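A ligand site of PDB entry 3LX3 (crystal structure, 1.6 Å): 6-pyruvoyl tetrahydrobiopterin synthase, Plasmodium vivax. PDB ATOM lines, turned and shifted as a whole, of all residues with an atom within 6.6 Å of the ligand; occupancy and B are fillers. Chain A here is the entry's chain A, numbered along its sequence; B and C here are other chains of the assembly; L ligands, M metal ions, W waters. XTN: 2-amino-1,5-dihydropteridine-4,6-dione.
An oxygen (O4) of the ligand sits at hydrogen-bond distance from the backbone NH of Thr 134 of chain B, at 2.8 Å.
The side-chain hydroxyl of Thr 134 of chain B sits at hydrogen-bond distance from an oxygen (O4) of the ligand, at 2.8 Å.
OE2 of Glu 135 of chain B is in hydrogen-bond range of N2 of the ligand.
OD1 of Asp 70 is in hydrogen-bond range of N8 of the ligand (2.8 Å).
A nitrogen (N2) of the ligand is in hydrogen-bond range of the backbone carbonyl oxygen (O) of Ile 69, at 2.8 Å.
N of Phe 71 sits at hydrogen-bond distance from N1 of the ligand (2.9 Å).
The side-chain hydroxyl of Tyr 67 sits close to a nitrogen (N8) of the ligand, 3.5 Å away.
OE2 of Glu 168 of chain B sits at hydrogen-bond distance from N5 of the ligand, at 3.4 Å.
The backbone NH of Val 68 is in hydrogen-bond range of the side-chain carboxylate of Glu 135 of chain B.
The side-chain carboxylate (OD1) of Asp 70 lies within hydrogen-bond range of the backbone NH (N) of Ser 72, 2.9 Å away.
OE1 of Glu 168 of chain B is in hydrogen-bond range of NE2 of Gln 172 of chain B, at 2.6 Å.
The side-chain carboxylate of Glu 168 of chain B lies close to a ring nitrogen (NE2) of His 36 of chain B (3.3 Å).
The side-chain hydroxyl (OG) of Ser 133 of chain B lies within hydrogen-bond range of the backbone carbonyl oxygen (O) of Gly 66, 2.7 Å away.
Residues that only touch the ligand: Leu 23 (3.7 Å) and Ser 133 of chain B (3.5 Å).
Water W2 lies within hydrogen-bond range of OE1 of Glu 168 of chain B (3.0 Å), O6 of the ligand (3.2 Å) and NE2 of His 87 of chain C (3.4 Å).
Water W1 lies within hydrogen-bond range of OE1 of Glu 45 of chain B (2.6 Å) and O6 of the ligand (3.4 Å).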
ATOM      1  N   LEU A  23      -6.552 -24.676 -15.649  1.00  0.00           N
ATOM      2  CA  LEU A  23      -6.143 -23.644 -16.574  1.00  0.00           C
ATOM      3  C   LEU A  23      -5.694 -22.408 -15.780  1.00  0.00           C
ATOM      4  O   LEU A  23      -6.307 -22.073 -14.740  1.00  0.00           O
ATOM      5  CB  LEU A  23      -7.276 -23.249 -17.480  1.00  0.00           C
ATOM      6  CG  LEU A  23      -7.825 -24.347 -18.369  1.00  0.00           C
ATOM      7  CD1 LEU A  23      -8.846 -23.760 -19.339  1.00  0.00           C
ATOM      8  CD2 LEU A  23      -6.767 -25.168 -19.092  1.00  0.00           C
ATOM      9  N   GLY A  66     -12.067 -30.377 -26.639  1.00  0.00           N
ATOM     10  CA  GLY A  66     -10.652 -30.316 -26.312  1.00  0.00           C
ATOM     11  C   GLY A  66     -10.200 -29.304 -25.267  1.00  0.00           C
ATOM     12  O   GLY A  66      -9.038 -29.261 -24.894  1.00  0.00           O
ATOM     13  N   TYR A  67     -11.145 -28.499 -24.808  1.00  0.00           N
ATOM     14  CA  TYR A  67     -10.912 -27.487 -23.794  1.00  0.00           C
ATOM     15  C   TYR A  67     -11.659 -27.776 -22.511  1.00  0.00           C
ATOM     16  O   TYR A  67     -12.749 -28.361 -22.565  1.00  0.00           O
ATOM     17  CB  TYR A  67     -11.446 -26.135 -24.261  1.00  0.00           C
ATOM     18  CG  TYR A  67     -10.858 -25.502 -25.524  1.00  0.00           C
ATOM     19  CD1 TYR A  67      -9.634 -25.883 -26.058  1.00  0.00           C
ATOM     20  CD2 TYR A  67     -11.600 -24.547 -26.190  1.00  0.00           C
ATOM     21  CE1 TYR A  67      -9.154 -25.258 -27.199  1.00  0.00           C
ATOM     22  CE2 TYR A  67     -11.114 -23.913 -27.314  1.00  0.00           C
ATOM     23  CZ  TYR A  67      -9.896 -24.266 -27.801  1.00  0.00           C
ATOM     24  OH  TYR A  67      -9.431 -23.626 -28.921  1.00  0.00           O
ATOM     25  N   VAL A  68     -11.114 -27.334 -21.373  1.00  0.00           N
ATOM     26  CA  VAL A  68     -11.959 -27.199 -20.178  1.00  0.00           C
ATOM     27  C   VAL A  68     -12.983 -26.094 -20.485  1.00  0.00           C
ATOM     28  O   VAL A  68     -14.207 -26.310 -20.423  1.00  0.00           O
ATOM     29  CB  VAL A  68     -11.201 -26.926 -18.897  1.00  0.00           C
ATOM     30  CG1 VAL A  68     -12.237 -26.758 -17.736  1.00  0.00           C
ATOM     31  CG2 VAL A  68     -10.250 -28.107 -18.609  1.00  0.00           C
ATOM     32  N   ILE A  69     -12.449 -24.933 -20.839  1.00  0.00           N
ATOM     33  CA  ILE A  69     -13.219 -23.731 -21.210  1.00  0.00           C
ATOM     34  C   ILE A  69     -12.222 -22.907 -22.052  1.00  0.00           C
ATOM     35  O   ILE A  69     -10.993 -22.939 -21.816  1.00  0.00           O
ATOM     36  CB  ILE A  69     -13.795 -23.017 -19.987  1.00  0.00           C
ATOM     37  CG1 ILE A  69     -14.573 -21.764 -20.381  1.00  0.00           C
ATOM     38  CG2 ILE A  69     -12.698 -22.678 -19.005  1.00  0.00           C
ATOM     39  CD1 ILE A  69     -15.340 -21.175 -19.195  1.00  0.00           C
ATOM     40  N   ASP A  70     -12.699 -22.250 -23.088  1.00  0.00           N
ATOM     41  CA  ASP A  70     -11.870 -21.495 -23.991  1.00  0.00           C
ATOM     42  C   ASP A  70     -11.101 -20.382 -23.266  1.00  0.00           C
ATOM     43  O   ASP A  70     -11.691 -19.479 -22.659  1.00  0.00           O
ATOM     44  CB  ASP A  70     -12.788 -20.889 -25.075  1.00  0.00           C
ATOM     45  CG  ASP A  70     -12.026 -20.238 -26.219  1.00  0.00           C
ATOM     46  OD1 ASP A  70     -10.822 -19.985 -26.141  1.00  0.00           O
ATOM     47  OD2 ASP A  70     -12.695 -19.984 -27.233  1.00  0.00           O
ATOM     48  N   PHE A  71      -9.767 -20.428 -23.338  1.00  0.00           N
ATOM     49  CA  PHE A  71      -8.935 -19.349 -22.781  1.00  0.00           C
ATOM     50  C   PHE A  71      -9.389 -17.963 -23.233  1.00  0.00           C
ATOM     51  O   PHE A  71      -9.264 -16.981 -22.473  1.00  0.00           O
ATOM     52  CB  PHE A  71      -7.459 -19.479 -23.209  1.00  0.00           C
ATOM     53  CG  PHE A  71      -6.650 -20.571 -22.520  1.00  0.00           C
ATOM     54  CD1 PHE A  71      -6.486 -20.629 -21.144  1.00  0.00           C
ATOM     55  CD2 PHE A  71      -5.923 -21.466 -23.294  1.00  0.00           C
ATOM     56  CE1 PHE A  71      -5.677 -21.621 -20.564  1.00  0.00           C
ATOM     57  CE2 PHE A  71      -5.118 -22.445 -22.685  1.00  0.00           C
ATOM     58  CZ  PHE A  71      -5.010 -22.495 -21.340  1.00  0.00           C
ATOM     59  N   SER A  72      -9.860 -17.823 -24.478  1.00  0.00           N
ATOM     60  CA  SER A  72     -10.212 -16.475 -24.981  1.00  0.00           C
ATOM     61  C   SER A  72     -11.357 -15.831 -24.186  1.00  0.00           C
ATOM     62  O   SER A  72     -11.383 -14.615 -23.984  1.00  0.00           O
ATOM     63  CB  SER A  72     -10.575 -16.541 -26.462  1.00  0.00           C
ATOM     64  OG  SER A  72      -9.502 -17.064 -27.224  1.00  0.00           O
ATOM     65  N   LEU A  74     -11.987 -16.510 -20.982  1.00  0.00           N
ATOM     66  CA  LEU A  74     -11.370 -16.155 -19.696  1.00  0.00           C
ATOM     67  C   LEU A  74     -10.636 -14.836 -19.787  1.00  0.00           C
ATOM     68  O   LEU A  74     -10.803 -13.947 -18.941  1.00  0.00           O
ATOM     69  CB  LEU A  74     -10.407 -17.236 -19.193  1.00  0.00           C
ATOM     70  CG  LEU A  74     -11.000 -18.637 -19.107  1.00  0.00           C
ATOM     71  CD1 LEU A  74      -9.989 -19.598 -18.459  1.00  0.00           C
ATOM     72  CD2 LEU A  74     -12.364 -18.638 -18.347  1.00  0.00           C
ATOM     73  N   HIS B  36       0.587 -25.644 -35.401  1.00  0.00           N
ATOM     74  CA  HIS B  36      -0.634 -26.384 -35.111  1.00  0.00           C
ATOM     75  C   HIS B  36      -1.837 -25.594 -35.621  1.00  0.00           C
ATOM     76  O   HIS B  36      -1.710 -24.439 -35.988  1.00  0.00           O
ATOM     77  CB  HIS B  36      -0.741 -26.711 -33.614  1.00  0.00           C
ATOM     78  CG  HIS B  36      -1.457 -25.686 -32.781  1.00  0.00           C
ATOM     79  ND1 HIS B  36      -2.509 -26.029 -31.964  1.00  0.00           N
ATOM     80  CD2 HIS B  36      -1.246 -24.360 -32.607  1.00  0.00           C
ATOM     81  CE1 HIS B  36      -2.924 -24.941 -31.322  1.00  0.00           C
ATOM     82  NE2 HIS B  36      -2.182 -23.909 -31.703  1.00  0.00           N
ATOM     83  N   ILE B  38      -6.128 -25.624 -34.008  1.00  0.00           N
ATOM     84  CA  ILE B  38      -7.285 -26.232 -33.327  1.00  0.00           C
ATOM     85  C   ILE B  38      -8.408 -26.463 -34.319  1.00  0.00           C
ATOM     86  O   ILE B  38      -8.727 -25.576 -35.126  1.00  0.00           O
ATOM     87  CB  ILE B  38      -7.835 -25.294 -32.224  1.00  0.00           C
ATOM     88  CG1 ILE B  38      -6.807 -25.072 -31.114  1.00  0.00           C
ATOM     89  CG2 ILE B  38      -9.199 -25.819 -31.669  1.00  0.00           C
ATOM     90  CD1 ILE B  38      -6.388 -26.298 -30.345  1.00  0.00           C
ATOM     91  N   PHE B  43     -15.724 -25.488 -35.637  1.00  0.00           N
ATOM     92  CA  PHE B  43     -14.641 -24.525 -35.490  1.00  0.00           C
ATOM     93  C   PHE B  43     -13.340 -25.039 -36.086  1.00  0.00           C
ATOM     94  O   PHE B  43     -12.943 -26.167 -35.803  1.00  0.00           O
ATOM     95  CB  PHE B  43     -14.417 -24.203 -34.021  1.00  0.00           C
ATOM     96  CG  PHE B  43     -13.302 -23.223 -33.778  1.00  0.00           C
ATOM     97  CD1 PHE B  43     -13.486 -21.866 -34.025  1.00  0.00           C
ATOM     98  CD2 PHE B  43     -12.069 -23.650 -33.308  1.00  0.00           C
ATOM     99  CE1 PHE B  43     -12.436 -20.967 -33.800  1.00  0.00           C
ATOM    100  CE2 PHE B  43     -11.029 -22.749 -33.093  1.00  0.00           C
ATOM    101  CZ  PHE B  43     -11.213 -21.423 -33.337  1.00  0.00           C
ATOM    102  N   GLU B  45      -9.419 -23.132 -36.920  1.00  0.00           N
ATOM    103  CA  GLU B  45      -8.631 -21.890 -37.026  1.00  0.00           C
ATOM    104  C   GLU B  45      -7.524 -22.049 -38.017  1.00  0.00           C
ATOM    105  O   GLU B  45      -7.248 -23.160 -38.473  1.00  0.00           O
ATOM    106  CB  GLU B  45      -8.093 -21.516 -35.688  1.00  0.00           C
ATOM    107  CG  GLU B  45      -7.033 -22.373 -35.226  1.00  0.00           C
ATOM    108  CD  GLU B  45      -6.591 -22.073 -33.795  1.00  0.00           C
ATOM    109  OE1 GLU B  45      -6.870 -20.974 -33.262  1.00  0.00           O
ATOM    110  OE2 GLU B  45      -5.910 -22.923 -33.221  1.00  0.00           O
ATOM    111  N   HIS B  48      -0.906 -21.759 -37.477  1.00  0.00           N
ATOM    112  CA  HIS B  48       0.003 -20.844 -36.805  1.00  0.00           C
ATOM    113  C   HIS B  48       0.953 -21.685 -35.939  1.00  0.00           C
ATOM    114  O   HIS B  48       1.167 -22.839 -36.224  1.00  0.00           O
ATOM    115  CB  HIS B  48      -0.813 -19.802 -36.005  1.00  0.00           C
ATOM    116  CG  HIS B  48      -1.603 -20.411 -34.897  1.00  0.00           C
ATOM    117  ND1 HIS B  48      -2.777 -21.129 -35.113  1.00  0.00           N
ATOM    118  CD2 HIS B  48      -1.356 -20.486 -33.586  1.00  0.00           C
ATOM    119  CE1 HIS B  48      -3.201 -21.607 -33.959  1.00  0.00           C
ATOM    120  NE2 HIS B  48      -2.362 -21.235 -32.990  1.00  0.00           N
ATOM    121  N   HIS B  50       3.616 -21.725 -32.031  1.00  0.00           N
ATOM    122  CA  HIS B  50       3.954 -21.321 -30.664  1.00  0.00           C
ATOM    123  C   HIS B  50       5.316 -21.851 -30.257  1.00  0.00           C
ATOM    124  O   HIS B  50       5.761 -22.900 -30.719  1.00  0.00           O
ATOM    125  CB  HIS B  50       2.960 -21.925 -29.700  1.00  0.00           C
ATOM    126  CG  HIS B  50       1.542 -21.526 -29.942  1.00  0.00           C
ATOM    127  ND1 HIS B  50       1.100 -20.235 -29.778  1.00  0.00           N
ATOM    128  CD2 HIS B  50       0.473 -22.246 -30.355  1.00  0.00           C
ATOM    129  CE1 HIS B  50      -0.180 -20.178 -30.080  1.00  0.00           C
ATOM    130  NE2 HIS B  50      -0.600 -21.381 -30.432  1.00  0.00           N
ATOM    131  N   SER B 132      -5.192 -30.540 -30.934  1.00  0.00           N
ATOM    132  CA  SER B 132      -3.942 -29.972 -30.470  1.00  0.00           C
ATOM    133  C   SER B 132      -4.126 -28.807 -29.476  1.00  0.00           C
ATOM    134  O   SER B 132      -3.528 -27.719 -29.616  1.00  0.00           O
ATOM    135  CB  SER B 132      -3.041 -29.597 -31.649  1.00  0.00           C
ATOM    136  OG  SER B 132      -3.706 -28.678 -32.509  1.00  0.00           O
ATOM    137  N   SER B 133      -4.964 -29.075 -28.465  1.00  0.00           N
ATOM    138  CA  SER B 133      -5.150 -28.123 -27.386  1.00  0.00           C
ATOM    139  C   SER B 133      -4.054 -28.270 -26.370  1.00  0.00           C
ATOM    140  O   SER B 133      -3.398 -29.318 -26.225  1.00  0.00           O
ATOM    141  CB  SER B 133      -6.504 -28.312 -26.733  1.00  0.00           C
ATOM    142  OG  SER B 133      -6.612 -29.590 -26.089  1.00  0.00           O
ATOM    143  N   THR B 134      -3.895 -27.198 -25.596  1.00  0.00           N
ATOM    144  CA  THR B 134      -2.927 -27.211 -24.534  1.00  0.00           C
ATOM    145  C   THR B 134      -3.143 -28.332 -23.524  1.00  0.00           C
ATOM    146  O   THR B 134      -2.211 -28.987 -23.108  1.00  0.00           O
ATOM    147  CB  THR B 134      -2.960 -25.804 -23.888  1.00  0.00           C
ATOM    148  OG1 THR B 134      -2.859 -24.793 -24.910  1.00  0.00           O
ATOM    149  CG2 THR B 134      -1.800 -25.642 -22.920  1.00  0.00           C
ATOM    150  N   GLU B 135      -4.409 -28.556 -23.186  1.00  0.00           N
ATOM    151  CA  GLU B 135      -4.840 -29.601 -22.282  1.00  0.00           C
ATOM    152  C   GLU B 135      -4.467 -30.992 -22.782  1.00  0.00           C
ATOM    153  O   GLU B 135      -3.878 -31.777 -22.034  1.00  0.00           O
ATOM    154  CB  GLU B 135      -6.348 -29.550 -22.085  1.00  0.00           C
ATOM    155  CG  GLU B 135      -6.921 -28.360 -21.335  1.00  0.00           C
ATOM    156  CD  GLU B 135      -7.368 -27.182 -22.235  1.00  0.00           C
ATOM    157  OE1 GLU B 135      -6.648 -26.865 -23.219  1.00  0.00           O
ATOM    158  OE2 GLU B 135      -8.403 -26.573 -21.868  1.00  0.00           O
ATOM    159  N   GLU B 168       0.946 -22.671 -24.399  1.00  0.00           N
ATOM    160  CA  GLU B 168       1.087 -22.260 -25.774  1.00  0.00           C
ATOM    161  C   GLU B 168       1.865 -20.941 -25.776  1.00  0.00           C
ATOM    162  O   GLU B 168       2.662 -20.723 -26.643  1.00  0.00           O
ATOM    163  CB  GLU B 168      -0.251 -21.900 -26.444  1.00  0.00           C
ATOM    164  CG  GLU B 168      -1.033 -22.951 -27.184  1.00  0.00           C
ATOM    165  CD  GLU B 168      -2.309 -22.338 -27.802  1.00  0.00           C
ATOM    166  OE1 GLU B 168      -2.607 -21.157 -27.479  1.00  0.00           O
ATOM    167  OE2 GLU B 168      -2.989 -22.976 -28.632  1.00  0.00           O
ATOM    168  N   GLN B 172      -1.196 -18.347 -21.116  1.00  0.00           N
ATOM    169  CA  GLN B 172      -2.239 -19.347 -21.012  1.00  0.00           C
ATOM    170  C   GLN B 172      -1.685 -20.755 -20.885  1.00  0.00           C
ATOM    171  O   GLN B 172      -0.972 -21.242 -21.790  1.00  0.00           O
ATOM    172  CB  GLN B 172      -3.211 -19.270 -22.174  1.00  0.00           C
ATOM    173  CG  GLN B 172      -2.641 -19.185 -23.518  1.00  0.00           C
ATOM    174  CD  GLN B 172      -3.720 -18.947 -24.597  1.00  0.00           C
ATOM    175  OE1 GLN B 172      -4.392 -17.920 -24.610  1.00  0.00           O
ATOM    176  NE2 GLN B 172      -3.880 -19.938 -25.505  1.00  0.00           N
ATOM    177  N   ALA B 174      -2.058 -24.893 -19.215  1.00  0.00           N
ATOM    178  CA  ALA B 174      -2.867 -25.997 -18.727  1.00  0.00           C
ATOM    179  C   ALA B 174      -1.990 -26.950 -17.945  1.00  0.00           C
ATOM    180  O   ALA B 174      -0.892 -27.281 -18.344  1.00  0.00           O
ATOM    181  CB  ALA B 174      -3.517 -26.757 -19.892  1.00  0.00           C
ATOM    182  N   HIS C  87      -1.311 -15.436 -36.179  1.00  0.00           N
ATOM    183  CA  HIS C  87      -2.190 -16.563 -36.498  1.00  0.00           C
ATOM    184  C   HIS C  87      -2.169 -16.903 -37.970  1.00  0.00           C
ATOM    185  O   HIS C  87      -3.152 -17.240 -38.569  1.00  0.00           O
ATOM    186  CB  HIS C  87      -3.637 -16.395 -36.029  1.00  0.00           C
ATOM    187  CG  HIS C  87      -3.927 -17.157 -34.789  1.00  0.00           C
ATOM    188  ND1 HIS C  87      -4.793 -18.216 -34.737  1.00  0.00           N
ATOM    189  CD2 HIS C  87      -3.365 -17.048 -33.559  1.00  0.00           C
ATOM    190  CE1 HIS C  87      -4.807 -18.708 -33.515  1.00  0.00           C
ATOM    191  NE2 HIS C  87      -3.958 -18.017 -32.780  1.00  0.00           N
HETATM  192  N1  XTN L   1      -8.536 -22.613 -24.869  1.00  0.00           N
HETATM  193  C2  XTN L   1      -8.104 -23.688 -24.169  1.00  0.00           C
HETATM  194  N2  XTN L   1      -8.724 -24.074 -23.043  1.00  0.00           N
HETATM  195  N3  XTN L   1      -7.013 -24.461 -24.659  1.00  0.00           N
HETATM  196  C4  XTN L   1      -6.339 -24.116 -25.758  1.00  0.00           C
HETATM  197  O4  XTN L   1      -5.357 -24.819 -26.106  1.00  0.00           O
HETATM  198  N5  XTN L   1      -6.165 -22.562 -27.580  1.00  0.00           N
HETATM  199  C6  XTN L   1      -6.626 -21.473 -28.255  1.00  0.00           C
HETATM  200  O6  XTN L   1      -6.072 -21.109 -29.289  1.00  0.00           O
HETATM  201  C7  XTN L   1      -7.778 -20.772 -27.767  1.00  0.00           C
HETATM  202  N8  XTN L   1      -8.354 -21.201 -26.646  1.00  0.00           N
HETATM  203  C4A XTN L   1      -6.779 -22.987 -26.437  1.00  0.00           C
HETATM  204  C8A XTN L   1      -7.881 -22.261 -25.978  1.00  0.00           C
HETATM  205 ZN    ZN M   1      -2.535 -21.940 -31.023  1.00  0.00          ZN
HETATM  206  O   HOH W   1      -8.502 -20.035 -31.472  1.00  0.00           O
HETATM  207  O   HOH W   2      -3.240 -20.053 -30.195  1.00  0.00           O
HETATM  208  O   HOH W   3      -4.554 -22.278 -31.043  1.00  0.00           O
